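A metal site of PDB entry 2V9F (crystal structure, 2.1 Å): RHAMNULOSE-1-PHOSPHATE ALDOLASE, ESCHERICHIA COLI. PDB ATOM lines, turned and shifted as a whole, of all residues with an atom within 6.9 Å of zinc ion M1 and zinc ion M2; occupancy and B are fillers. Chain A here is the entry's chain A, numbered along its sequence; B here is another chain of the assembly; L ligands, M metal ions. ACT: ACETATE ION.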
ATOM      1  N   TRP A  25      -8.103  -6.115  21.869  1.00  0.00           N
ATOM      2  CA  TRP A  25      -8.350  -7.496  22.231  1.00  0.00           C
ATOM      3  C   TRP A  25      -7.359  -8.052  23.242  1.00  0.00           C
ATOM      4  O   TRP A  25      -7.634  -9.078  23.874  1.00  0.00           O
ATOM      5  CB  TRP A  25      -8.240  -8.413  21.010  1.00  0.00           C
ATOM      6  CG  TRP A  25      -9.181  -8.150  19.883  1.00  0.00           C
ATOM      7  CD1 TRP A  25     -10.340  -7.433  19.925  1.00  0.00           C
ATOM      8  CD2 TRP A  25      -9.060  -8.646  18.550  1.00  0.00           C
ATOM      9  NE1 TRP A  25     -10.953  -7.469  18.694  1.00  0.00           N
ATOM     10  CE2 TRP A  25     -10.186  -8.212  17.832  1.00  0.00           C
ATOM     11  CE3 TRP A  25      -8.097  -9.434  17.892  1.00  0.00           C
ATOM     12  CZ2 TRP A  25     -10.382  -8.521  16.486  1.00  0.00           C
ATOM     13  CZ3 TRP A  25      -8.289  -9.750  16.552  1.00  0.00           C
ATOM     14  CH2 TRP A  25      -9.430  -9.290  15.868  1.00  0.00           C
ATOM     15  N   ASP A  26      -6.203  -7.412  23.368  1.00  0.00           N
ATOM     16  CA  ASP A  26      -5.188  -7.941  24.255  1.00  0.00           C
ATOM     17  C   ASP A  26      -4.613  -6.981  25.269  1.00  0.00           C
ATOM     18  O   ASP A  26      -3.482  -6.526  25.139  1.00  0.00           O
ATOM     19  CB  ASP A  26      -4.059  -8.542  23.423  1.00  0.00           C
ATOM     20  CG  ASP A  26      -4.555  -9.602  22.448  1.00  0.00           C
ATOM     21  OD1 ASP A  26      -5.240  -9.248  21.471  1.00  0.00           O
ATOM     22  OD2 ASP A  26      -4.261 -10.797  22.675  1.00  0.00           O
ATOM     23  N   GLU A  27      -5.402  -6.655  26.270  1.00  0.00           N
ATOM     24  CA  GLU A  27      -4.939  -5.776  27.316  1.00  0.00           C
ATOM     25  C   GLU A  27      -4.002  -6.590  28.185  1.00  0.00           C
ATOM     26  O   GLU A  27      -4.128  -7.823  28.288  1.00  0.00           O
ATOM     27  CB  GLU A  27      -6.115  -5.272  28.172  1.00  0.00           C
ATOM     28  CG  GLU A  27      -6.941  -6.384  28.769  1.00  0.00           C
ATOM     29  CD  GLU A  27      -7.754  -7.134  27.735  1.00  0.00           C
ATOM     30  OE1 GLU A  27      -8.310  -8.184  28.071  1.00  0.00           O
ATOM     31  OE2 GLU A  27      -7.859  -6.681  26.561  1.00  0.00           O
ATOM     32  N   ARG A  28      -3.053  -5.891  28.804  1.00  0.00           N
ATOM     33  CA  ARG A  28      -2.102  -6.514  29.699  1.00  0.00           C
ATOM     34  C   ARG A  28      -1.495  -7.723  29.021  1.00  0.00           C
ATOM     35  O   ARG A  28      -0.944  -7.608  27.922  1.00  0.00           O
ATOM     36  CB  ARG A  28      -2.814  -6.923  30.985  1.00  0.00           C
ATOM     37  CG  ARG A  28      -1.881  -7.260  32.135  1.00  0.00           C
ATOM     38  CD  ARG A  28      -2.657  -7.400  33.431  1.00  0.00           C
ATOM     39  NE  ARG A  28      -1.745  -7.569  34.561  1.00  0.00           N
ATOM     40  CZ  ARG A  28      -1.050  -8.679  34.802  1.00  0.00           C
ATOM     41  NH1 ARG A  28      -1.164  -9.730  34.005  1.00  0.00           N
ATOM     42  NH2 ARG A  28      -0.215  -8.720  35.829  1.00  0.00           N
ATOM     43  N   ASN A  29      -1.618  -8.883  29.661  1.00  0.00           N
ATOM     44  CA  ASN A  29      -1.068 -10.141  29.151  1.00  0.00           C
ATOM     45  C   ASN A  29      -2.199 -11.022  28.642  1.00  0.00           C
ATOM     46  O   ASN A  29      -2.012 -12.233  28.434  1.00  0.00           O
ATOM     47  CB  ASN A  29      -0.348 -10.877  30.266  1.00  0.00           C
ATOM     48  CG  ASN A  29      -1.307 -11.331  31.366  1.00  0.00           C
ATOM     49  OD1 ASN A  29      -2.157 -10.563  31.820  1.00  0.00           O
ATOM     50  ND2 ASN A  29      -1.188 -12.592  31.783  1.00  0.00           N
ATOM     51  N   GLY A  30      -3.381 -10.433  28.468  1.00  0.00           N
ATOM     52  CA  GLY A  30      -4.516 -11.200  27.982  1.00  0.00           C
ATOM     53  C   GLY A  30      -4.308 -11.555  26.523  1.00  0.00           C
ATOM     54  O   GLY A  30      -4.252 -10.677  25.665  1.00  0.00           O
ATOM     55  N   GLY A  31      -4.186 -12.837  26.223  1.00  0.00           N
ATOM     56  CA  GLY A  31      -3.992 -13.246  24.842  1.00  0.00           C
ATOM     57  C   GLY A  31      -2.656 -13.933  24.591  1.00  0.00           C
ATOM     58  O   GLY A  31      -1.669 -13.703  25.308  1.00  0.00           O
ATOM     59  N   ASN A  32      -2.621 -14.786  23.580  1.00  0.00           N
ATOM     60  CA  ASN A  32      -1.392 -15.489  23.241  1.00  0.00           C
ATOM     61  C   ASN A  32      -1.439 -16.028  21.813  1.00  0.00           C
ATOM     62  O   ASN A  32      -2.505 -16.253  21.237  1.00  0.00           O
ATOM     63  CB  ASN A  32      -1.127 -16.610  24.265  1.00  0.00           C
ATOM     64  CG  ASN A  32      -2.362 -17.000  25.045  1.00  0.00           C
ATOM     65  OD1 ASN A  32      -3.180 -17.787  24.581  1.00  0.00           O
ATOM     66  ND2 ASN A  32      -2.517 -16.424  26.249  1.00  0.00           N
ATOM     67  N   GLU A 117      -0.793 -20.655  28.620  1.00  0.00           N
ATOM     68  CA  GLU A 117      -1.860 -21.307  27.859  1.00  0.00           C
ATOM     69  C   GLU A 117      -1.292 -22.257  26.821  1.00  0.00           C
ATOM     70  O   GLU A 117      -2.022 -22.744  25.947  1.00  0.00           O
ATOM     71  CB  GLU A 117      -2.759 -20.261  27.162  1.00  0.00           C
ATOM     72  CG  GLU A 117      -3.641 -19.485  28.139  1.00  0.00           C
ATOM     73  CD  GLU A 117      -4.472 -20.403  29.032  1.00  0.00           C
ATOM     74  OE1 GLU A 117      -4.963 -19.920  30.072  1.00  0.00           O
ATOM     75  OE2 GLU A 117      -4.637 -21.601  28.710  1.00  0.00           O
ATOM     76  N   HIS A 141      -5.111 -16.809  20.440  1.00  0.00           N
ATOM     77  CA  HIS A 141      -6.051 -16.551  21.493  1.00  0.00           C
ATOM     78  C   HIS A 141      -6.100 -15.058  21.788  1.00  0.00           C
ATOM     79  O   HIS A 141      -5.074 -14.416  21.946  1.00  0.00           O
ATOM     80  CB  HIS A 141      -5.650 -17.304  22.764  1.00  0.00           C
ATOM     81  CG  HIS A 141      -6.473 -16.941  23.955  1.00  0.00           C
ATOM     82  ND1 HIS A 141      -7.853 -17.037  23.973  1.00  0.00           N
ATOM     83  CD2 HIS A 141      -6.120 -16.497  25.188  1.00  0.00           C
ATOM     84  CE1 HIS A 141      -8.304 -16.654  25.149  1.00  0.00           C
ATOM     85  NE2 HIS A 141      -7.270 -16.327  25.902  1.00  0.00           N
ATOM     86  N   CYS A 142      -7.303 -14.524  21.874  1.00  0.00           N
ATOM     87  CA  CYS A 142      -7.434 -13.113  22.167  1.00  0.00           C
ATOM     88  C   CYS A 142      -8.733 -12.880  22.893  1.00  0.00           C
ATOM     89  O   CYS A 142      -9.664 -13.683  22.811  1.00  0.00           O
ATOM     90  CB  CYS A 142      -7.372 -12.292  20.889  1.00  0.00           C
ATOM     91  SG  CYS A 142      -8.870 -12.355  19.953  1.00  0.00           S
ATOM     92  N   HIS A 143      -8.772 -11.782  23.629  1.00  0.00           N
ATOM     93  CA  HIS A 143      -9.954 -11.430  24.386  1.00  0.00           C
ATOM     94  C   HIS A 143     -10.813 -10.463  23.605  1.00  0.00           C
ATOM     95  O   HIS A 143     -10.908  -9.290  23.949  1.00  0.00           O
ATOM     96  CB  HIS A 143      -9.525 -10.848  25.724  1.00  0.00           C
ATOM     97  CG  HIS A 143      -8.726 -11.806  26.549  1.00  0.00           C
ATOM     98  ND1 HIS A 143      -8.285 -11.502  27.821  1.00  0.00           N
ATOM     99  CD2 HIS A 143      -8.293 -13.052  26.284  1.00  0.00           C
ATOM    100  CE1 HIS A 143      -7.604 -12.529  28.302  1.00  0.00           C
ATOM    101  NE2 HIS A 143      -7.588 -13.488  27.382  1.00  0.00           N
ATOM    102  N   ILE A 148     -16.872 -11.948  23.908  1.00  0.00           N
ATOM    103  CA  ILE A 148     -16.922 -12.174  25.347  1.00  0.00           C
ATOM    104  C   ILE A 148     -18.272 -11.692  25.876  1.00  0.00           C
ATOM    105  O   ILE A 148     -18.984 -12.448  26.540  1.00  0.00           O
ATOM    106  CB  ILE A 148     -15.761 -11.416  26.066  1.00  0.00           C
ATOM    107  CG1 ILE A 148     -14.427 -12.104  25.725  1.00  0.00           C
ATOM    108  CG2 ILE A 148     -15.994 -11.406  27.583  1.00  0.00           C
ATOM    109  CD1 ILE A 148     -13.192 -11.309  26.089  1.00  0.00           C
ATOM    110  N   PRO A 188      -8.441 -21.474  33.402  1.00  0.00           N
ATOM    111  CA  PRO A 188      -7.471 -21.314  32.313  1.00  0.00           C
ATOM    112  C   PRO A 188      -6.073 -21.778  32.723  1.00  0.00           C
ATOM    113  O   PRO A 188      -5.794 -21.935  33.916  1.00  0.00           O
ATOM    114  CB  PRO A 188      -7.542 -19.811  32.011  1.00  0.00           C
ATOM    115  CG  PRO A 188      -7.818 -19.218  33.363  1.00  0.00           C
ATOM    116  CD  PRO A 188      -8.842 -20.170  33.960  1.00  0.00           C
ATOM    117  N   TRP A 209     -14.210 -19.444  24.932  1.00  0.00           N
ATOM    118  CA  TRP A 209     -14.061 -19.736  26.341  1.00  0.00           C
ATOM    119  C   TRP A 209     -15.002 -18.684  26.941  1.00  0.00           C
ATOM    120  O   TRP A 209     -14.668 -17.501  26.984  1.00  0.00           O
ATOM    121  CB  TRP A 209     -12.631 -19.500  26.791  1.00  0.00           C
ATOM    122  CG  TRP A 209     -11.666 -20.526  26.354  1.00  0.00           C
ATOM    123  CD1 TRP A 209     -11.914 -21.648  25.595  1.00  0.00           C
ATOM    124  CD2 TRP A 209     -10.288 -20.611  26.749  1.00  0.00           C
ATOM    125  NE1 TRP A 209     -10.779 -22.421  25.514  1.00  0.00           N
ATOM    126  CE2 TRP A 209      -9.772 -21.811  26.210  1.00  0.00           C
ATOM    127  CE3 TRP A 209      -9.447 -19.783  27.526  1.00  0.00           C
ATOM    128  CZ2 TRP A 209      -8.441 -22.209  26.421  1.00  0.00           C
ATOM    129  CZ3 TRP A 209      -8.122 -20.183  27.724  1.00  0.00           C
ATOM    130  CH2 TRP A 209      -7.633 -21.381  27.172  1.00  0.00           C
ATOM    131  N   HIS A 212     -14.260 -15.252  28.902  1.00  0.00           N
ATOM    132  CA  HIS A 212     -12.817 -15.187  28.833  1.00  0.00           C
ATOM    133  C   HIS A 212     -12.333 -14.718  27.467  1.00  0.00           C
ATOM    134  O   HIS A 212     -11.738 -13.639  27.363  1.00  0.00           O
ATOM    135  CB  HIS A 212     -12.242 -16.583  29.200  1.00  0.00           C
ATOM    136  CG  HIS A 212     -10.749 -16.609  29.300  1.00  0.00           C
ATOM    137  ND1 HIS A 212     -10.079 -17.507  30.107  1.00  0.00           N
ATOM    138  CD2 HIS A 212      -9.803 -15.861  28.703  1.00  0.00           C
ATOM    139  CE1 HIS A 212      -8.779 -17.306  29.996  1.00  0.00           C
ATOM    140  NE2 HIS A 212      -8.588 -16.313  29.156  1.00  0.00           N
ATOM    141  N   GLY A 213     -12.591 -15.496  26.414  1.00  0.00           N
ATOM    142  CA  GLY A 213     -12.119 -15.094  25.095  1.00  0.00           C
ATOM    143  C   GLY A 213     -12.348 -16.075  23.979  1.00  0.00           C
ATOM    144  O   GLY A 213     -13.269 -16.891  24.030  1.00  0.00           O
ATOM    145  N   VAL A 214     -11.483 -16.017  22.958  1.00  0.00           N
ATOM    146  CA  VAL A 214     -11.621 -16.871  21.777  1.00  0.00           C
ATOM    147  C   VAL A 214     -10.292 -17.473  21.326  1.00  0.00           C
ATOM    148  O   VAL A 214      -9.222 -16.879  21.517  1.00  0.00           O
ATOM    149  CB  VAL A 214     -12.253 -16.030  20.607  1.00  0.00           C
ATOM    150  CG1 VAL A 214     -11.276 -14.979  20.117  1.00  0.00           C
ATOM    151  CG2 VAL A 214     -12.657 -16.925  19.450  1.00  0.00           C
ATOM    152  N   PHE A 215     -10.371 -18.668  20.745  1.00  0.00           N
ATOM    153  CA  PHE A 215      -9.215 -19.393  20.200  1.00  0.00           C
ATOM    154  C   PHE A 215      -9.516 -19.632  18.729  1.00  0.00           C
ATOM    155  O   PHE A 215     -10.631 -20.004  18.371  1.00  0.00           O
ATOM    156  CB  PHE A 215      -9.015 -20.760  20.890  1.00  0.00           C
ATOM    157  CG  PHE A 215      -8.036 -20.733  22.018  1.00  0.00           C
ATOM    158  CD1 PHE A 215      -8.371 -20.160  23.234  1.00  0.00           C
ATOM    159  CD2 PHE A 215      -6.745 -21.228  21.843  1.00  0.00           C
ATOM    160  CE1 PHE A 215      -7.432 -20.077  24.259  1.00  0.00           C
ATOM    161  CE2 PHE A 215      -5.797 -21.143  22.865  1.00  0.00           C
ATOM    162  CZ  PHE A 215      -6.144 -20.565  24.078  1.00  0.00           C
ATOM    163  N   SER B 169     -14.468 -10.509  33.046  1.00  0.00           N
ATOM    164  CA  SER B 169     -13.280 -11.011  32.337  1.00  0.00           C
ATOM    165  C   SER B 169     -12.615 -11.968  33.300  1.00  0.00           C
ATOM    166  O   SER B 169     -12.312 -11.600  34.444  1.00  0.00           O
ATOM    167  CB  SER B 169     -12.309  -9.875  31.964  1.00  0.00           C
ATOM    168  OG  SER B 169     -12.765  -9.148  30.821  1.00  0.00           O
ATOM    169  N   THR B 170     -12.403 -13.203  32.859  1.00  0.00           N
ATOM    170  CA  THR B 170     -11.815 -14.235  33.721  1.00  0.00           C
ATOM    171  C   THR B 170     -10.526 -13.883  34.470  1.00  0.00           C
ATOM    172  O   THR B 170     -10.405 -14.168  35.662  1.00  0.00           O
ATOM    173  CB  THR B 170     -11.563 -15.541  32.916  1.00  0.00           C
ATOM    174  OG1 THR B 170     -12.822 -16.110  32.557  1.00  0.00           O
ATOM    175  CG2 THR B 170     -10.742 -16.574  33.731  1.00  0.00           C
ATOM    176  N   GLU B 171      -9.572 -13.257  33.796  1.00  0.00           N
ATOM    177  CA  GLU B 171      -8.304 -12.924  34.448  1.00  0.00           C
ATOM    178  C   GLU B 171      -8.381 -11.848  35.532  1.00  0.00           C
ATOM    179  O   GLU B 171      -7.412 -11.658  36.266  1.00  0.00           O
ATOM    180  CB  GLU B 171      -7.289 -12.458  33.417  1.00  0.00           C
ATOM    181  CG  GLU B 171      -7.505 -11.030  33.008  1.00  0.00           C
ATOM    182  CD  GLU B 171      -8.302 -10.903  31.726  1.00  0.00           C
ATOM    183  OE1 GLU B 171      -9.151 -11.783  31.416  1.00  0.00           O
ATOM    184  OE2 GLU B 171      -8.097  -9.892  31.045  1.00  0.00           O
ATOM    185  N   CYS B 172      -9.496 -11.144  35.626  1.00  0.00           N
ATOM    186  CA  CYS B 172      -9.614 -10.062  36.603  1.00  0.00           C
ATOM    187  C   CYS B 172      -9.317 -10.446  38.034  1.00  0.00           C
ATOM    188  O   CYS B 172      -8.556  -9.751  38.729  1.00  0.00           O
ATOM    189  CB  CYS B 172     -10.989  -9.398  36.509  1.00  0.00           C
ATOM    190  SG  CYS B 172     -11.130  -8.359  35.016  1.00  0.00           S
ATOM    191  N   THR B 230      -7.071  -3.822  32.315  1.00  0.00           N
ATOM    192  CA  THR B 230      -7.799  -5.059  32.554  1.00  0.00           C
ATOM    193  C   THR B 230      -9.153  -4.736  33.187  1.00  0.00           C
ATOM    194  O   THR B 230     -10.182  -5.300  32.805  1.00  0.00           O
ATOM    195  CB  THR B 230      -6.981  -6.013  33.462  1.00  0.00           C
ATOM    196  OG1 THR B 230      -5.785  -6.405  32.779  1.00  0.00           O
ATOM    197  CG2 THR B 230      -7.785  -7.259  33.813  1.00  0.00           C
ATOM    198  N   LYS B 233     -11.305  -3.067  30.597  1.00  0.00           N
ATOM    199  CA  LYS B 233     -11.720  -4.044  29.593  1.00  0.00           C
ATOM    200  C   LYS B 233     -12.943  -4.800  30.119  1.00  0.00           C
ATOM    201  O   LYS B 233     -13.926  -5.000  29.398  1.00  0.00           O
ATOM    202  CB  LYS B 233     -10.591  -5.035  29.290  1.00  0.00           C
ATOM    203  CG  LYS B 233     -11.005  -6.301  28.535  1.00  0.00           C
ATOM    204  CD  LYS B 233     -11.768  -6.000  27.265  1.00  0.00           C
ATOM    205  CE  LYS B 233     -11.696  -7.164  26.266  1.00  0.00           C
ATOM    206  NZ  LYS B 233     -10.387  -7.156  25.525  1.00  0.00           N
ATOM    207  N   SER B 234     -12.879  -5.197  31.386  1.00  0.00           N
ATOM    208  CA  SER B 234     -13.995  -5.901  31.990  1.00  0.00           C
ATOM    209  C   SER B 234     -15.187  -4.953  32.048  1.00  0.00           C
ATOM    210  O   SER B 234     -16.308  -5.348  31.747  1.00  0.00           O
ATOM    211  CB  SER B 234     -13.630  -6.394  33.396  1.00  0.00           C
ATOM    212  OG  SER B 234     -14.727  -7.080  33.976  1.00  0.00           O
HETATM  213  C   ACT L   1      -4.625 -15.377  28.971  1.00  0.00           C
HETATM  214  O   ACT L   1      -5.615 -14.985  29.624  1.00  0.00           O
HETATM  215  OXT ACT L   1      -4.682 -15.715  27.773  1.00  0.00           O
HETATM  216  CH3 ACT L   1      -3.278 -15.461  29.687  1.00  0.00           C
HETATM  217 ZN    ZN M   1      -8.699  -9.854  29.021  1.00  0.00          ZN
HETATM  218 ZN    ZN M   2      -7.025 -15.435  27.871  1.00  0.00          ZN
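The side-chain amino group (NZ) of Lys 233 of chain B lies within salt-bridge range of the side-chain carboxylate (OE2) of Glu 27, 2.8 Å away. The backbone carbonyl oxygen (O) of His 143 lies within hydrogen-bond range of the side-chain amino group (NZ) of Lys 233 of chain B. The backbone NH of His 143 lies within hydrogen-bond range of the backbone carbonyl oxygen of Trp 25 (2.9 Å). O of Asn 32 is in hydrogen-bond range of N of His 141 (2.8 Å). ND1 of His 141 is in hydrogen-bond range of O of Val 214 (2.8 Å).
Of the 26 residues printed, 3 come within 4 Å of zinc ion M1.
Three residues have an atom within 4 Å of zinc ion M2: His 141, His 143 and His 212.
OE1 of Glu 27 binds zinc ion M1 (2.0 Å). A ring nitrogen (ND1) of His 143 binds zinc ion M1, 2.1 Å away. Zinc ion M1 is bound by OE2 of Glu 171 of chain B, at 2.1 Å.
Zinc ion M2 is bound by NE2 of His 143, NE2 of His 141, NE2 of His 212, O of the ligand and OXT of the ligand. Zinc ion M2 has five donor atoms within binding distance.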
